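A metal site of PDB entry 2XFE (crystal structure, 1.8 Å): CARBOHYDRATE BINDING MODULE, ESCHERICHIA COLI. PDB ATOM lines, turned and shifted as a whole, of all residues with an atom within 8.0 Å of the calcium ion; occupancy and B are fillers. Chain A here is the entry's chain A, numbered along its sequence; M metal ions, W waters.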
ATOM      1  N   ARG A   8     -30.523  18.265 -18.552  1.00  0.00           N
ATOM      2  CA  ARG A   8     -30.203  17.953 -17.133  1.00  0.00           C
ATOM      3  C   ARG A   8     -28.677  17.787 -17.033  1.00  0.00           C
ATOM      4  O   ARG A   8     -28.074  16.889 -17.606  1.00  0.00           O
ATOM      5  CB  ARG A   8     -30.900  16.693 -16.675  1.00  0.00           C
ATOM      6  CG  ARG A   8     -30.488  16.393 -15.224  1.00  0.00           C
ATOM      7  CD  ARG A   8     -31.668  16.058 -14.412  1.00  0.00           C
ATOM      8  NE  ARG A   8     -31.410  15.846 -12.969  1.00  0.00           N
ATOM      9  CZ  ARG A   8     -31.952  16.591 -12.033  1.00  0.00           C
ATOM     10  NH1 ARG A   8     -31.712  16.289 -10.769  1.00  0.00           N
ATOM     11  NH2 ARG A   8     -32.746  17.576 -12.360  1.00  0.00           N
ATOM     12  N   MET A  36     -26.849  18.539 -10.284  1.00  0.00           N
ATOM     13  CA  MET A  36     -27.650  18.211 -11.424  1.00  0.00           C
ATOM     14  C   MET A  36     -28.967  18.962 -11.300  1.00  0.00           C
ATOM     15  O   MET A  36     -29.665  18.844 -10.281  1.00  0.00           O
ATOM     16  CB  MET A  36     -27.910  16.683 -11.513  1.00  0.00           C
ATOM     17  CG  MET A  36     -26.827  15.849 -12.141  1.00  0.00           C
ATOM     18  SD  MET A  36     -26.693  16.251 -13.862  1.00  0.00           S
ATOM     19  CE  MET A  36     -25.390  15.102 -14.242  1.00  0.00           C
ATOM     20  N   GLN A  63     -20.992  17.574 -16.925  1.00  0.00           N
ATOM     21  CA  GLN A  63     -21.685  16.312 -16.940  1.00  0.00           C
ATOM     22  C   GLN A  63     -23.120  16.568 -17.325  1.00  0.00           C
ATOM     23  O   GLN A  63     -23.879  17.351 -16.699  1.00  0.00           O
ATOM     24  CB  GLN A  63     -21.587  15.613 -15.587  1.00  0.00           C
ATOM     25  CG  GLN A  63     -22.053  14.189 -15.600  1.00  0.00           C
ATOM     26  CD  GLN A  63     -22.285  13.610 -14.155  1.00  0.00           C
ATOM     27  OE1 GLN A  63     -22.188  14.326 -13.147  1.00  0.00           O
ATOM     28  NE2 GLN A  63     -22.683  12.330 -14.115  1.00  0.00           N
ATOM     29  N   VAL A  64     -23.522  15.904 -18.406  1.00  0.00           N
ATOM     30  CA  VAL A  64     -24.894  16.019 -18.898  1.00  0.00           C
ATOM     31  C   VAL A  64     -25.494  14.646 -18.666  1.00  0.00           C
ATOM     32  O   VAL A  64     -24.989  13.639 -19.165  1.00  0.00           O
ATOM     33  CB  VAL A  64     -24.957  16.398 -20.410  1.00  0.00           C
ATOM     34  CG1 VAL A  64     -26.365  16.398 -20.874  1.00  0.00           C
ATOM     35  CG2 VAL A  64     -24.311  17.719 -20.657  1.00  0.00           C
ATOM     36  N   ASP A  65     -26.541  14.561 -17.841  1.00  0.00           N
ATOM     37  CA  ASP A  65     -27.180  13.269 -17.590  1.00  0.00           C
ATOM     38  C   ASP A  65     -27.974  12.804 -18.814  1.00  0.00           C
ATOM     39  O   ASP A  65     -27.770  11.701 -19.312  1.00  0.00           O
ATOM     40  CB  ASP A  65     -28.114  13.430 -16.367  1.00  0.00           C
ATOM     41  CG  ASP A  65     -28.648  12.125 -15.847  1.00  0.00           C
ATOM     42  OD1 ASP A  65     -28.530  11.068 -16.495  1.00  0.00           O
ATOM     43  OD2 ASP A  65     -29.116  12.161 -14.719  1.00  0.00           O
ATOM     44  N   TYR A  66     -28.853  13.681 -19.271  1.00  0.00           N
ATOM     45  CA  TYR A  66     -29.754  13.474 -20.366  1.00  0.00           C
ATOM     46  C   TYR A  66     -30.329  14.772 -20.853  1.00  0.00           C
ATOM     47  O   TYR A  66     -30.209  15.809 -20.230  1.00  0.00           O
ATOM     48  CB  TYR A  66     -30.924  12.500 -19.992  1.00  0.00           C
ATOM     49  CG  TYR A  66     -31.762  12.935 -18.799  1.00  0.00           C
ATOM     50  CD1 TYR A  66     -32.764  13.858 -18.939  1.00  0.00           C
ATOM     51  CD2 TYR A  66     -31.500  12.415 -17.540  1.00  0.00           C
ATOM     52  CE1 TYR A  66     -33.529  14.257 -17.835  1.00  0.00           C
ATOM     53  CE2 TYR A  66     -32.215  12.804 -16.417  1.00  0.00           C
ATOM     54  CZ  TYR A  66     -33.267  13.719 -16.588  1.00  0.00           C
ATOM     55  OH  TYR A  66     -34.022  14.182 -15.524  1.00  0.00           O
ATOM     56  N   ILE A  67     -31.020  14.689 -21.995  1.00  0.00           N
ATOM     57  CA  ILE A  67     -31.962  15.743 -22.391  1.00  0.00           C
ATOM     58  C   ILE A  67     -33.332  15.080 -22.621  1.00  0.00           C
ATOM     59  O   ILE A  67     -33.430  13.846 -22.717  1.00  0.00           O
ATOM     60  CB  ILE A  67     -31.523  16.543 -23.631  1.00  0.00           C
ATOM     61  CG1 ILE A  67     -31.701  15.712 -24.897  1.00  0.00           C
ATOM     62  CG2 ILE A  67     -30.066  17.034 -23.447  1.00  0.00           C
ATOM     63  CD1 ILE A  67     -31.434  16.468 -26.206  1.00  0.00           C
ATOM     64  N   THR A  73     -37.051  11.147 -23.489  1.00  0.00           N
ATOM     65  CA  THR A  73     -35.701  11.163 -22.894  1.00  0.00           C
ATOM     66  C   THR A  73     -34.592  10.643 -23.832  1.00  0.00           C
ATOM     67  O   THR A  73     -34.771   9.614 -24.472  1.00  0.00           O
ATOM     68  CB  THR A  73     -35.719  10.431 -21.556  1.00  0.00           C
ATOM     69  OG1 THR A  73     -36.610  11.121 -20.646  1.00  0.00           O
ATOM     70  CG2 THR A  73     -34.352  10.417 -20.958  1.00  0.00           C
ATOM     71  N   ARG A  74     -33.441  11.323 -23.862  1.00  0.00           N
ATOM     72  CA  ARG A  74     -32.279  10.912 -24.605  1.00  0.00           C
ATOM     73  C   ARG A  74     -31.079  10.967 -23.646  1.00  0.00           C
ATOM     74  O   ARG A  74     -30.682  12.035 -23.242  1.00  0.00           O
ATOM     75  CB  ARG A  74     -32.038  11.821 -25.810  1.00  0.00           C
ATOM     76  CG  ARG A  74     -33.201  11.891 -26.756  1.00  0.00           C
ATOM     77  CD  ARG A  74     -32.883  12.652 -27.996  1.00  0.00           C
ATOM     78  NE  ARG A  74     -34.112  12.866 -28.765  1.00  0.00           N
ATOM     79  CZ  ARG A  74     -34.181  13.552 -29.892  1.00  0.00           C
ATOM     80  NH1 ARG A  74     -33.092  14.046 -30.436  1.00  0.00           N
ATOM     81  NH2 ARG A  74     -35.375  13.734 -30.496  1.00  0.00           N
ATOM     82  N   GLN A  75     -30.551   9.816 -23.273  1.00  0.00           N
ATOM     83  CA  GLN A  75     -29.411   9.746 -22.334  1.00  0.00           C
ATOM     84  C   GLN A  75     -28.138  10.191 -22.994  1.00  0.00           C
ATOM     85  O   GLN A  75     -27.853   9.798 -24.108  1.00  0.00           O
ATOM     86  CB  GLN A  75     -29.215   8.314 -21.807  1.00  0.00           C
ATOM     87  CG  GLN A  75     -30.365   7.777 -20.929  1.00  0.00           C
ATOM     88  CD  GLN A  75     -30.557   8.489 -19.622  1.00  0.00           C
ATOM     89  OE1 GLN A  75     -29.620   9.097 -19.103  1.00  0.00           O
ATOM     90  NE2 GLN A  75     -31.757   8.390 -19.064  1.00  0.00           N
ATOM     91  N   ALA A  76     -27.352  11.018 -22.302  1.00  0.00           N
ATOM     92  CA  ALA A  76     -26.092  11.547 -22.927  1.00  0.00           C
ATOM     93  C   ALA A  76     -25.181  10.316 -23.247  1.00  0.00           C
ATOM     94  O   ALA A  76     -24.566  10.297 -24.298  1.00  0.00           O
ATOM     95  CB  ALA A  76     -25.394  12.551 -21.979  1.00  0.00           C
ATOM     96  N   GLU A  77     -25.222   9.292 -22.382  1.00  0.00           N
ATOM     97  CA  GLU A  77     -24.369   8.133 -22.508  1.00  0.00           C
ATOM     98  C   GLU A  77     -24.775   7.146 -23.598  1.00  0.00           C
ATOM     99  O   GLU A  77     -23.987   6.252 -23.940  1.00  0.00           O
ATOM    100  CB  GLU A  77     -24.185   7.412 -21.160  1.00  0.00           C
ATOM    101  CG  GLU A  77     -25.417   6.869 -20.557  1.00  0.00           C
ATOM    102  CD  GLU A  77     -26.171   7.863 -19.667  1.00  0.00           C
ATOM    103  OE1 GLU A  77     -26.709   7.459 -18.617  1.00  0.00           O
ATOM    104  OE2 GLU A  77     -26.296   9.030 -20.028  1.00  0.00           O
ATOM    105  N   ASN A  78     -25.946   7.360 -24.178  1.00  0.00           N
ATOM    106  CA  ASN A  78     -26.366   6.627 -25.357  1.00  0.00           C
ATOM    107  C   ASN A  78     -26.072   7.306 -26.650  1.00  0.00           C
ATOM    108  O   ASN A  78     -26.454   6.800 -27.688  1.00  0.00           O
ATOM    109  CB  ASN A  78     -27.852   6.292 -25.274  1.00  0.00           C
ATOM    110  CG  ASN A  78     -28.158   5.302 -24.184  1.00  0.00           C
ATOM    111  OD1 ASN A  78     -27.255   4.644 -23.638  1.00  0.00           O
ATOM    112  ND2 ASN A  78     -29.409   5.226 -23.819  1.00  0.00           N
ATOM    113  N   SER A  97     -20.726   8.944 -23.455  1.00  0.00           N
ATOM    114  CA  SER A  97     -20.336   9.417 -22.128  1.00  0.00           C
ATOM    115  C   SER A  97     -21.189  10.591 -21.749  1.00  0.00           C
ATOM    116  O   SER A  97     -21.568  11.392 -22.584  1.00  0.00           O
ATOM    117  CB  SER A  97     -18.868   9.874 -22.102  1.00  0.00           C
ATOM    118  OG  SER A  97     -18.480  10.302 -20.771  1.00  0.00           O
ATOM    119  N   GLU A  98     -21.473  10.730 -20.449  1.00  0.00           N
ATOM    120  CA  GLU A  98     -22.116  11.915 -19.932  1.00  0.00           C
ATOM    121  C   GLU A  98     -21.207  13.142 -19.847  1.00  0.00           C
ATOM    122  O   GLU A  98     -21.673  14.262 -19.648  1.00  0.00           O
ATOM    123  CB  GLU A  98     -22.610  11.618 -18.506  1.00  0.00           C
ATOM    124  CG  GLU A  98     -23.706  10.594 -18.472  1.00  0.00           C
ATOM    125  CD  GLU A  98     -24.387  10.469 -17.121  1.00  0.00           C
ATOM    126  OE1 GLU A  98     -23.750  10.569 -16.048  1.00  0.00           O
ATOM    127  OE2 GLU A  98     -25.575  10.274 -17.064  1.00  0.00           O
HETATM  128 CA    CA M   1     -27.657   9.629 -18.032  1.00  0.00          CA
HETATM  129  O   HOH W   1     -28.519   8.138 -16.421  1.00  0.00           O
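The backbone NH of Ala 76 lies close to the backbone carbonyl oxygen of Asp 65 (3.1 Å).
The backbone NH (N) of Asp 65 sits at hydrogen-bond distance from the backbone carbonyl oxygen (O) of Arg 8 (2.8 Å).
The backbone carbonyl oxygen (O) of Glu 98 lies within hydrogen-bond range of the backbone NH (N) of Val 64.
The side-chain carboxylate (OE1) of Glu 98 sits at hydrogen-bond distance from the side-chain amide nitrogen (NE2) of Gln 63 (2.8 Å).
Within 4 Å of the calcium ion: Asp 65, Gln 75, Glu 77 and Glu 98.
The nearest printed residue that does not touch the calcium ion is Tyr 66 (4.4 Å).
The calcium ion is bound by the side-chain carboxylate (OD1) of Asp 65 (2.3 Å), the side-chain amide oxygen (OE1) of Gln 75 (2.3 Å), water W1 (2.4 Å), the side-chain carboxylate (OE2) of Glu 98 (2.4 Å), the backbone carbonyl oxygen (O) of Asp 65 (2.4 Å), the side-chain carboxylate (OE1) of Glu 77 (2.4 Å) and the side-chain carboxylate (OE2) of Glu 77 (2.5 Å).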
